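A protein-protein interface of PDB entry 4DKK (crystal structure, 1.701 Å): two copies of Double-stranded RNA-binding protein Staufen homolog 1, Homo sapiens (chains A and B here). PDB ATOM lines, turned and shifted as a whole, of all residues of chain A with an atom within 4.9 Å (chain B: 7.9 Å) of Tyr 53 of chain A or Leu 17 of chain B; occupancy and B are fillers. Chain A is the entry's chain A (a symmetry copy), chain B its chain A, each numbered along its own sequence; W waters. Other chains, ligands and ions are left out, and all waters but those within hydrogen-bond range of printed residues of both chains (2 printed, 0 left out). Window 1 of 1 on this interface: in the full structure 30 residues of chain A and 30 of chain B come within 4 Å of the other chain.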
ATOM      1  N   LEU A  44      35.262  23.461 -13.067  1.00  0.00           N
ATOM      2  CA  LEU A  44      34.272  22.818 -13.914  1.00  0.00           C
ATOM      3  C   LEU A  44      33.736  23.863 -14.850  1.00  0.00           C
ATOM      4  O   LEU A  44      33.041  24.806 -14.448  1.00  0.00           O
ATOM      5  CB  LEU A  44      33.141  22.261 -13.062  1.00  0.00           C
ATOM      6  CG  LEU A  44      33.522  21.126 -12.127  1.00  0.00           C
ATOM      7  CD1 LEU A  44      32.390  20.874 -11.151  1.00  0.00           C
ATOM      8  CD2 LEU A  44      33.853  19.859 -12.916  1.00  0.00           C
ATOM      9  N   GLU A  49      28.243  20.713 -15.843  1.00  0.00           N
ATOM     10  CA  GLU A  49      29.175  20.148 -14.881  1.00  0.00           C
ATOM     11  C   GLU A  49      29.032  20.842 -13.547  1.00  0.00           C
ATOM     12  O   GLU A  49      29.022  20.201 -12.491  1.00  0.00           O
ATOM     13  CB  GLU A  49      30.610  20.301 -15.399  1.00  0.00           C
ATOM     14  CG  GLU A  49      30.876  19.540 -16.690  1.00  0.00           C
ATOM     15  CD  GLU A  49      32.216  19.904 -17.352  1.00  0.00           C
ATOM     16  OE1 GLU A  49      32.720  21.042 -17.220  1.00  0.00           O
ATOM     17  OE2 GLU A  49      32.777  19.012 -18.010  1.00  0.00           O
ATOM     18  N   GLN A  50      28.959  22.163 -13.595  1.00  0.00           N
ATOM     19  CA  GLN A  50      28.789  22.951 -12.373  1.00  0.00           C
ATOM     20  C   GLN A  50      27.535  22.502 -11.609  1.00  0.00           C
ATOM     21  O   GLN A  50      27.586  22.291 -10.394  1.00  0.00           O
ATOM     22  CB  GLN A  50      28.707  24.431 -12.716  1.00  0.00           C
ATOM     23  CG  GLN A  50      30.037  24.972 -13.220  1.00  0.00           C
ATOM     24  CD  GLN A  50      29.905  26.299 -13.926  1.00  0.00           C
ATOM     25  OE1 GLN A  50      28.835  26.925 -13.924  1.00  0.00           O
ATOM     26  NE2 GLN A  50      30.993  26.731 -14.575  1.00  0.00           N
ATOM     27  N   LEU A  51      26.410  22.377 -12.312  1.00  0.00           N
ATOM     28  CA  LEU A  51      25.165  21.977 -11.676  1.00  0.00           C
ATOM     29  C   LEU A  51      25.226  20.536 -11.132  1.00  0.00           C
ATOM     30  O   LEU A  51      24.729  20.266 -10.025  1.00  0.00           O
ATOM     31  CB  LEU A  51      23.984  22.159 -12.622  1.00  0.00           C
ATOM     32  CG  LEU A  51      22.603  21.795 -12.050  1.00  0.00           C
ATOM     33  CD1 LEU A  51      22.273  22.578 -10.801  1.00  0.00           C
ATOM     34  CD2 LEU A  51      21.545  22.011 -13.113  1.00  0.00           C
ATOM     35  N   ASP A  52      25.847  19.624 -11.878  1.00  0.00           N
ATOM     36  CA  ASP A  52      26.066  18.217 -11.418  1.00  0.00           C
ATOM     37  C   ASP A  52      26.802  18.258 -10.071  1.00  0.00           C
ATOM     38  O   ASP A  52      26.397  17.612  -9.098  1.00  0.00           O
ATOM     39  CB  ASP A  52      26.899  17.553 -12.515  1.00  0.00           C
ATOM     40  CG  ASP A  52      27.027  16.061 -12.420  1.00  0.00           C
ATOM     41  OD1 ASP A  52      26.540  15.410 -11.469  1.00  0.00           O
ATOM     42  OD2 ASP A  52      27.681  15.548 -13.381  1.00  0.00           O
ATOM     43  N   TYR A  53      27.860  19.063  -9.984  1.00  0.00           N
ATOM     44  CA  TYR A  53      28.624  19.191  -8.733  1.00  0.00           C
ATOM     45  C   TYR A  53      27.795  19.768  -7.584  1.00  0.00           C
ATOM     46  O   TYR A  53      27.805  19.238  -6.481  1.00  0.00           O
ATOM     47  CB  TYR A  53      29.853  20.052  -8.999  1.00  0.00           C
ATOM     48  CG  TYR A  53      30.800  20.306  -7.853  1.00  0.00           C
ATOM     49  CD1 TYR A  53      31.514  19.278  -7.260  1.00  0.00           C
ATOM     50  CD2 TYR A  53      31.042  21.593  -7.424  1.00  0.00           C
ATOM     51  CE1 TYR A  53      32.430  19.549  -6.234  1.00  0.00           C
ATOM     52  CE2 TYR A  53      31.942  21.868  -6.430  1.00  0.00           C
ATOM     53  CZ  TYR A  53      32.626  20.860  -5.831  1.00  0.00           C
ATOM     54  OH  TYR A  53      33.526  21.180  -4.839  1.00  0.00           O
ATOM     55  N   LEU A  54      27.077  20.857  -7.842  1.00  0.00           N
ATOM     56  CA  LEU A  54      26.240  21.460  -6.824  1.00  0.00           C
ATOM     57  C   LEU A  54      25.227  20.424  -6.290  1.00  0.00           C
ATOM     58  O   LEU A  54      25.004  20.287  -5.078  1.00  0.00           O
ATOM     59  CB  LEU A  54      25.513  22.671  -7.416  1.00  0.00           C
ATOM     60  CG  LEU A  54      24.444  23.377  -6.574  1.00  0.00           C
ATOM     61  CD1 LEU A  54      24.945  23.922  -5.264  1.00  0.00           C
ATOM     62  CD2 LEU A  54      23.863  24.529  -7.399  1.00  0.00           C
ATOM     63  N   SER A  55      24.645  19.675  -7.213  1.00  0.00           N
ATOM     64  CA  SER A  55      23.603  18.724  -6.827  1.00  0.00           C
ATOM     65  C   SER A  55      24.208  17.629  -5.986  1.00  0.00           C
ATOM     66  O   SER A  55      23.597  17.140  -5.031  1.00  0.00           O
ATOM     67  CB  SER A  55      22.931  18.164  -8.071  1.00  0.00           C
ATOM     68  OG  SER A  55      23.636  17.068  -8.558  1.00  0.00           O
ATOM     69  N   ARG A  56      25.414  17.226  -6.328  1.00  0.00           N
ATOM     70  CA  ARG A  56      26.087  16.195  -5.561  1.00  0.00           C
ATOM     71  C   ARG A  56      26.337  16.622  -4.110  1.00  0.00           C
ATOM     72  O   ARG A  56      26.123  15.837  -3.196  1.00  0.00           O
ATOM     73  CB  ARG A  56      27.377  15.786  -6.249  1.00  0.00           C
ATOM     74  CG  ARG A  56      28.217  14.806  -5.474  1.00  0.00           C
ATOM     75  CD  ARG A  56      29.680  14.980  -5.849  1.00  0.00           C
ATOM     76  NE  ARG A  56      30.579  14.479  -4.814  1.00  0.00           N
ATOM     77  CZ  ARG A  56      31.876  14.762  -4.754  1.00  0.00           C
ATOM     78  NH1 ARG A  56      32.436  15.548  -5.672  1.00  0.00           N
ATOM     79  NH2 ARG A  56      32.612  14.266  -3.770  1.00  0.00           N
ATOM     80  N   VAL A  57      26.779  17.864  -3.890  1.00  0.00           N
ATOM     81  CA  VAL A  57      27.019  18.357  -2.547  1.00  0.00           C
ATOM     82  C   VAL A  57      25.731  18.568  -1.781  1.00  0.00           C
ATOM     83  O   VAL A  57      25.621  18.167  -0.621  1.00  0.00           O
ATOM     84  CB  VAL A  57      27.753  19.714  -2.567  1.00  0.00           C
ATOM     85  CG1 VAL A  57      28.084  20.136  -1.146  1.00  0.00           C
ATOM     86  CG2 VAL A  57      28.996  19.610  -3.404  1.00  0.00           C
ATOM     87  N   THR B  10      23.051  26.942  -0.841  1.00  0.00           N
ATOM     88  CA  THR B  10      22.908  26.598  -2.256  1.00  0.00           C
ATOM     89  C   THR B  10      23.188  27.795  -3.159  1.00  0.00           C
ATOM     90  O   THR B  10      23.877  27.666  -4.175  1.00  0.00           O
ATOM     91  CB  THR B  10      21.509  26.061  -2.544  1.00  0.00           C
ATOM     92  OG1 THR B  10      21.333  24.839  -1.820  1.00  0.00           O
ATOM     93  CG2 THR B  10      21.310  25.828  -4.036  1.00  0.00           C
ATOM     94  N   ALA B  11      22.650  28.963  -2.816  1.00  0.00           N
ATOM     95  CA  ALA B  11      22.917  30.158  -3.623  1.00  0.00           C
ATOM     96  C   ALA B  11      24.409  30.513  -3.647  1.00  0.00           C
ATOM     97  O   ALA B  11      24.954  30.909  -4.689  1.00  0.00           O
ATOM     98  CB  ALA B  11      22.101  31.330  -3.117  1.00  0.00           C
ATOM     99  N   MET B  12      25.086  30.324  -2.521  1.00  0.00           N
ATOM    100  CA  MET B  12      26.497  30.691  -2.409  1.00  0.00           C
ATOM    101  C   MET B  12      27.339  29.800  -3.311  1.00  0.00           C
ATOM    102  O   MET B  12      28.204  30.278  -4.025  1.00  0.00           O
ATOM    103  CB  MET B  12      26.981  30.592  -0.948  1.00  0.00           C
ATOM    104  CG  MET B  12      26.410  31.653  -0.024  1.00  0.00           C
ATOM    105  SD  MET B  12      27.012  31.381   1.655  1.00  0.00           S
ATOM    106  CE  MET B  12      28.697  30.943   1.243  1.00  0.00           C
ATOM    107  N   ILE B  13      27.076  28.499  -3.254  1.00  0.00           N
ATOM    108  CA  ILE B  13      27.778  27.539  -4.088  1.00  0.00           C
ATOM    109  C   ILE B  13      27.491  27.828  -5.559  1.00  0.00           C
ATOM    110  O   ILE B  13      28.399  27.860  -6.401  1.00  0.00           O
ATOM    111  CB  ILE B  13      27.385  26.102  -3.745  1.00  0.00           C
ATOM    112  CG1 ILE B  13      27.822  25.775  -2.312  1.00  0.00           C
ATOM    113  CG2 ILE B  13      28.015  25.144  -4.728  1.00  0.00           C
ATOM    114  CD1 ILE B  13      27.181  24.483  -1.778  1.00  0.00           C
ATOM    115  N   ALA B  14      26.228  28.070  -5.890  1.00  0.00           N
ATOM    116  CA  ALA B  14      25.888  28.272  -7.290  1.00  0.00           C
ATOM    117  C   ALA B  14      26.585  29.515  -7.827  1.00  0.00           C
ATOM    118  O   ALA B  14      27.101  29.499  -8.964  1.00  0.00           O
ATOM    119  CB  ALA B  14      24.381  28.394  -7.469  1.00  0.00           C
ATOM    120  N   ARG B  15      26.619  30.565  -7.012  1.00  0.00           N
ATOM    121  CA  ARG B  15      27.266  31.825  -7.421  1.00  0.00           C
ATOM    122  C   ARG B  15      28.765  31.626  -7.657  1.00  0.00           C
ATOM    123  O   ARG B  15      29.327  32.138  -8.606  1.00  0.00           O
ATOM    124  CB  ARG B  15      27.066  32.923  -6.404  1.00  0.00           C
ATOM    125  CG  ARG B  15      25.663  33.485  -6.418  1.00  0.00           C
ATOM    126  CD  ARG B  15      25.511  34.522  -5.394  1.00  0.00           C
ATOM    127  NE  ARG B  15      24.135  34.982  -5.352  1.00  0.00           N
ATOM    128  CZ  ARG B  15      23.750  36.118  -4.802  1.00  0.00           C
ATOM    129  NH1 ARG B  15      24.639  36.943  -4.225  1.00  0.00           N
ATOM    130  NH2 ARG B  15      22.462  36.441  -4.813  1.00  0.00           N
ATOM    131  N   GLU B  16      29.409  30.915  -6.748  1.00  0.00           N
ATOM    132  CA  GLU B  16      30.831  30.643  -6.877  1.00  0.00           C
ATOM    133  C   GLU B  16      31.118  29.870  -8.174  1.00  0.00           C
ATOM    134  O   GLU B  16      32.122  30.129  -8.867  1.00  0.00           O
ATOM    135  CB  GLU B  16      31.335  29.836  -5.659  1.00  0.00           C
ATOM    136  CG  GLU B  16      31.413  30.663  -4.383  1.00  0.00           C
ATOM    137  CD  GLU B  16      31.537  29.849  -3.095  1.00  0.00           C
ATOM    138  OE1 GLU B  16      31.751  28.620  -3.142  1.00  0.00           O
ATOM    139  OE2 GLU B  16      31.440  30.479  -2.017  1.00  0.00           O
ATOM    140  N   LEU B  17      30.272  28.887  -8.485  1.00  0.00           N
ATOM    141  CA  LEU B  17      30.443  28.109  -9.705  1.00  0.00           C
ATOM    142  C   LEU B  17      30.226  28.970 -10.944  1.00  0.00           C
ATOM    143  O   LEU B  17      30.998  28.910 -11.903  1.00  0.00           O
ATOM    144  CB  LEU B  17      29.496  26.907  -9.737  1.00  0.00           C
ATOM    145  CG  LEU B  17      29.859  25.869  -8.670  1.00  0.00           C
ATOM    146  CD1 LEU B  17      28.712  24.883  -8.473  1.00  0.00           C
ATOM    147  CD2 LEU B  17      31.153  25.148  -9.038  1.00  0.00           C
ATOM    148  N   LEU B  18      29.152  29.750 -10.932  1.00  0.00           N
ATOM    149  CA  LEU B  18      28.863  30.635 -12.064  1.00  0.00           C
ATOM    150  C   LEU B  18      29.990  31.616 -12.288  1.00  0.00           C
ATOM    151  O   LEU B  18      30.308  31.932 -13.441  1.00  0.00           O
ATOM    152  CB  LEU B  18      27.583  31.407 -11.834  1.00  0.00           C
ATOM    153  CG  LEU B  18      26.313  30.594 -12.099  1.00  0.00           C
ATOM    154  CD1 LEU B  18      25.113  31.461 -11.828  1.00  0.00           C
ATOM    155  CD2 LEU B  18      26.255  29.981 -13.504  1.00  0.00           C
ATOM    156  N   TYR B  19      30.602  32.082 -11.214  1.00  0.00           N
ATOM    157  CA  TYR B  19      31.620  33.103 -11.357  1.00  0.00           C
ATOM    158  C   TYR B  19      32.925  32.490 -11.841  1.00  0.00           C
ATOM    159  O   TYR B  19      33.583  33.033 -12.762  1.00  0.00           O
ATOM    160  CB  TYR B  19      31.884  33.901 -10.044  1.00  0.00           C
ATOM    161  CG  TYR B  19      32.960  34.900 -10.301  1.00  0.00           C
ATOM    162  CD1 TYR B  19      32.687  36.096 -10.928  1.00  0.00           C
ATOM    163  CD2 TYR B  19      34.269  34.593 -10.001  1.00  0.00           C
ATOM    164  CE1 TYR B  19      33.712  36.964 -11.228  1.00  0.00           C
ATOM    165  CE2 TYR B  19      35.261  35.412 -10.286  1.00  0.00           C
ATOM    166  CZ  TYR B  19      35.012  36.595 -10.909  1.00  0.00           C
ATOM    167  OH  TYR B  19      36.106  37.400 -11.134  1.00  0.00           O
ATOM    168  N   GLY B  20      33.315  31.379 -11.215  1.00  0.00           N
ATOM    169  CA  GLY B  20      34.648  30.831 -11.444  1.00  0.00           C
ATOM    170  C   GLY B  20      34.847  29.354 -11.626  1.00  0.00           C
ATOM    171  O   GLY B  20      36.001  28.886 -11.681  1.00  0.00           O
ATOM    172  N   GLY B  21      33.761  28.605 -11.678  1.00  0.00           N
ATOM    173  CA  GLY B  21      33.848  27.188 -11.950  1.00  0.00           C
ATOM    174  C   GLY B  21      34.467  26.404 -10.816  1.00  0.00           C
ATOM    175  O   GLY B  21      34.892  25.272 -11.007  1.00  0.00           O
ATOM    176  N   THR B  22      34.503  26.995  -9.628  1.00  0.00           N
ATOM    177  CA  THR B  22      34.950  26.283  -8.428  1.00  0.00           C
ATOM    178  C   THR B  22      34.074  26.767  -7.284  1.00  0.00           C
ATOM    179  O   THR B  22      33.428  27.794  -7.396  1.00  0.00           O
ATOM    180  CB  THR B  22      36.409  26.584  -8.042  1.00  0.00           C
ATOM    181  OG1 THR B  22      36.527  27.954  -7.633  1.00  0.00           O
ATOM    182  CG2 THR B  22      37.312  26.351  -9.205  1.00  0.00           C
ATOM    183  N   SER B  23      34.067  26.035  -6.184  1.00  0.00           N
ATOM    184  CA  SER B  23      33.274  26.462  -5.043  1.00  0.00           C
ATOM    185  C   SER B  23      34.007  26.206  -3.750  1.00  0.00           C
ATOM    186  O   SER B  23      33.982  25.101  -3.227  1.00  0.00           O
ATOM    187  CB  SER B  23      31.904  25.742  -4.999  1.00  0.00           C
ATOM    188  OG  SER B  23      31.238  26.144  -3.816  1.00  0.00           O
ATOM    189  N   PRO B  24      34.659  27.238  -3.197  1.00  0.00           N
ATOM    190  CA  PRO B  24      35.297  27.026  -1.896  1.00  0.00           C
ATOM    191  C   PRO B  24      34.299  26.580  -0.826  1.00  0.00           C
ATOM    192  O   PRO B  24      34.652  25.795   0.071  1.00  0.00           O
ATOM    193  CB  PRO B  24      35.895  28.402  -1.563  1.00  0.00           C
ATOM    194  CG  PRO B  24      35.997  29.101  -2.869  1.00  0.00           C
ATOM    195  CD  PRO B  24      34.954  28.565  -3.766  1.00  0.00           C
ATOM    196  N   THR B  25      33.058  27.045  -0.927  1.00  0.00           N
ATOM    197  CA  THR B  25      32.035  26.644   0.037  1.00  0.00           C
ATOM    198  C   THR B  25      31.764  25.148  -0.072  1.00  0.00           C
ATOM    199  O   THR B  25      31.696  24.457   0.935  1.00  0.00           O
ATOM    200  CB  THR B  25      30.759  27.490  -0.164  1.00  0.00           C
ATOM    201  OG1 THR B  25      31.077  28.859   0.126  1.00  0.00           O
ATOM    202  CG2 THR B  25      29.599  27.017   0.741  1.00  0.00           C
ATOM    203  N   ALA B  26      31.663  24.627  -1.286  1.00  0.00           N
ATOM    204  CA  ALA B  26      31.404  23.196  -1.448  1.00  0.00           C
ATOM    205  C   ALA B  26      32.615  22.422  -0.976  1.00  0.00           C
ATOM    206  O   ALA B  26      32.506  21.365  -0.369  1.00  0.00           O
ATOM    207  CB  ALA B  26      31.151  22.873  -2.877  1.00  0.00           C
ATOM    208  N   GLU B  27      33.780  22.945  -1.256  1.00  0.00           N
ATOM    209  CA  GLU B  27      35.015  22.296  -0.864  1.00  0.00           C
ATOM    210  C   GLU B  27      35.104  22.189   0.640  1.00  0.00           C
ATOM    211  O   GLU B  27      35.586  21.223   1.150  1.00  0.00           O
ATOM    212  CB  GLU B  27      36.228  23.046  -1.365  1.00  0.00           C
ATOM    213  CG  GLU B  27      36.545  22.759  -2.790  1.00  0.00           C
ATOM    214  CD  GLU B  27      37.637  23.658  -3.340  1.00  0.00           C
ATOM    215  OE1 GLU B  27      38.691  23.734  -2.688  1.00  0.00           O
ATOM    216  OE2 GLU B  27      37.468  24.245  -4.415  1.00  0.00           O
ATOM    217  N   THR B  28      34.644  23.195   1.329  1.00  0.00           N
ATOM    218  CA  THR B  28      34.682  23.173   2.800  1.00  0.00           C
ATOM    219  C   THR B  28      33.726  22.100   3.346  1.00  0.00           C
ATOM    220  O   THR B  28      34.051  21.378   4.281  1.00  0.00           O
ATOM    221  CB  THR B  28      34.363  24.574   3.408  1.00  0.00           C
ATOM    222  OG1 THR B  28      35.392  25.499   3.044  1.00  0.00           O
ATOM    223  CG2 THR B  28      34.305  24.520   4.932  1.00  0.00           C
ATOM    224  N   ILE B  29      32.566  21.985   2.712  1.00  0.00           N
ATOM    225  CA  ILE B  29      31.532  21.044   3.123  1.00  0.00           C
ATOM    226  C   ILE B  29      31.991  19.598   3.035  1.00  0.00           C
ATOM    227  O   ILE B  29      31.743  18.825   3.947  1.00  0.00           O
ATOM    228  CB  ILE B  29      30.234  21.243   2.292  1.00  0.00           C
ATOM    229  CG1 ILE B  29      29.588  22.577   2.680  1.00  0.00           C
ATOM    230  CG2 ILE B  29      29.258  20.088   2.508  1.00  0.00           C
ATOM    231  CD1 ILE B  29      28.459  23.042   1.757  1.00  0.00           C
ATOM    232  N   LEU B  30      32.648  19.213   1.950  1.00  0.00           N
ATOM    233  CA  LEU B  30      33.229  17.980   1.432  1.00  0.00           C
ATOM    234  C   LEU B  30      34.580  17.666   2.063  1.00  0.00           C
ATOM    235  O   LEU B  30      34.965  16.500   2.132  1.00  0.00           O
ATOM    236  CB  LEU B  30      33.348  18.022  -0.081  1.00  0.00           C
ATOM    237  CG  LEU B  30      32.019  18.127  -0.830  1.00  0.00           C
ATOM    238  CD1 LEU B  30      32.306  18.262  -2.312  1.00  0.00           C
ATOM    239  CD2 LEU B  30      31.125  16.930  -0.554  1.00  0.00           C
HETATM  240  O   HOH W   1      35.219  23.418  -6.216  1.00  0.00           O
HETATM  241  O   HOH W   2      31.751  29.539 -14.738  1.00  0.00           O
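The side-chain amide nitrogen (NE2) of Gln 50 of chain A sits at hydrogen-bond distance from the backbone carbonyl oxygen (O) of Leu 17 of chain B.
N of Leu 44 of chain A lies within hydrogen-bond range of O of Gly 21 of chain B.
Of chain B, only Leu 17 (3.9 Å), Ala 26 (3.5 Å) and Glu 27 (3.98 Å) come within 4 Å of Tyr 53 of chain A.
Leu 17 of chain B touches just these residues of chain A: Gln 50 (3.4 Å) and Tyr 53 (3.9 Å).
Printed residues of chain A within 4 Å of Gly 21 of chain B: Leu 44 (2.8 Å) and Gln 50 (3.9 Å).
Of the printed residues of chain B, Gln 50 of chain A touches Leu 17 (3.4 Å) and Gly 21 (3.9 Å).
Of the printed residues of chain B, Leu 44 of chain A touches Gly 21.
The nearest printed residue of chain A that does not touch Ala 14 of chain B is Gln 50 of chain A (5.9 Å).
No position is printed for both chains.
Of the 11 pairs that touch across the chains among the printed residues, none has its exchanged pair printed and touching as well.
Of the 21 printed residues of chain B, 8 touch a printed residue of chain A.
Hydrophobic or aromatic side chains of chain B within 4 Å of the printed part of chain A: Ile 13, Ala 14, Leu 17, Ala 26, Ile 29 and Leu 30.
Of the 10 printed residues of chain A, 5 touch a printed residue of chain B.
Water W1 lies within hydrogen-bond range of N of Ser 23 of chain B, OE2 of Glu 27 of chain B and OH of Tyr 53 of chain A.
Water W2 lies within hydrogen-bond range of NE2 of Gln 50 of chain A (2.9 Å), O of Leu 17 of chain B (3.0 Å) and O of Leu 18 of chain B (3.1 Å).
The backbone NH (N) of Ala 26 of chain B is in hydrogen-bond range of the side-chain hydroxyl (OG) of Ser 23 of chain B, at 3.0 Å.
The backbone carbonyl oxygen (O) of Leu 44 of chain A sits at hydrogen-bond distance from the side-chain amide nitrogen (NE2) of Gln 50 of chain A, 2.8 Å away.
Among the printed residues, pairs that only touch across the chains: Leu 54 of chain A with Ile 13 of chain B (3.3 Å), Tyr 53 of chain A with Ala 26 of chain B (3.5 Å), Val 57 of chain A with Leu 30 of chain B (3.7 Å), Val 57 of chain A with Ile 29 of chain B (3.8 Å), Leu 54 of chain A with Ala 14 of chain B (3.9 Å), Gln 50 of chain A with Gly 21 of chain B (3.9 Å), Tyr 53 of chain A with Leu 17 of chain B (3.9 Å), Val 57 of chain A with Ala 26 of chain B (3.9 Å) and Tyr 53 of chain A with Glu 27 of chain B (3.98 Å).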
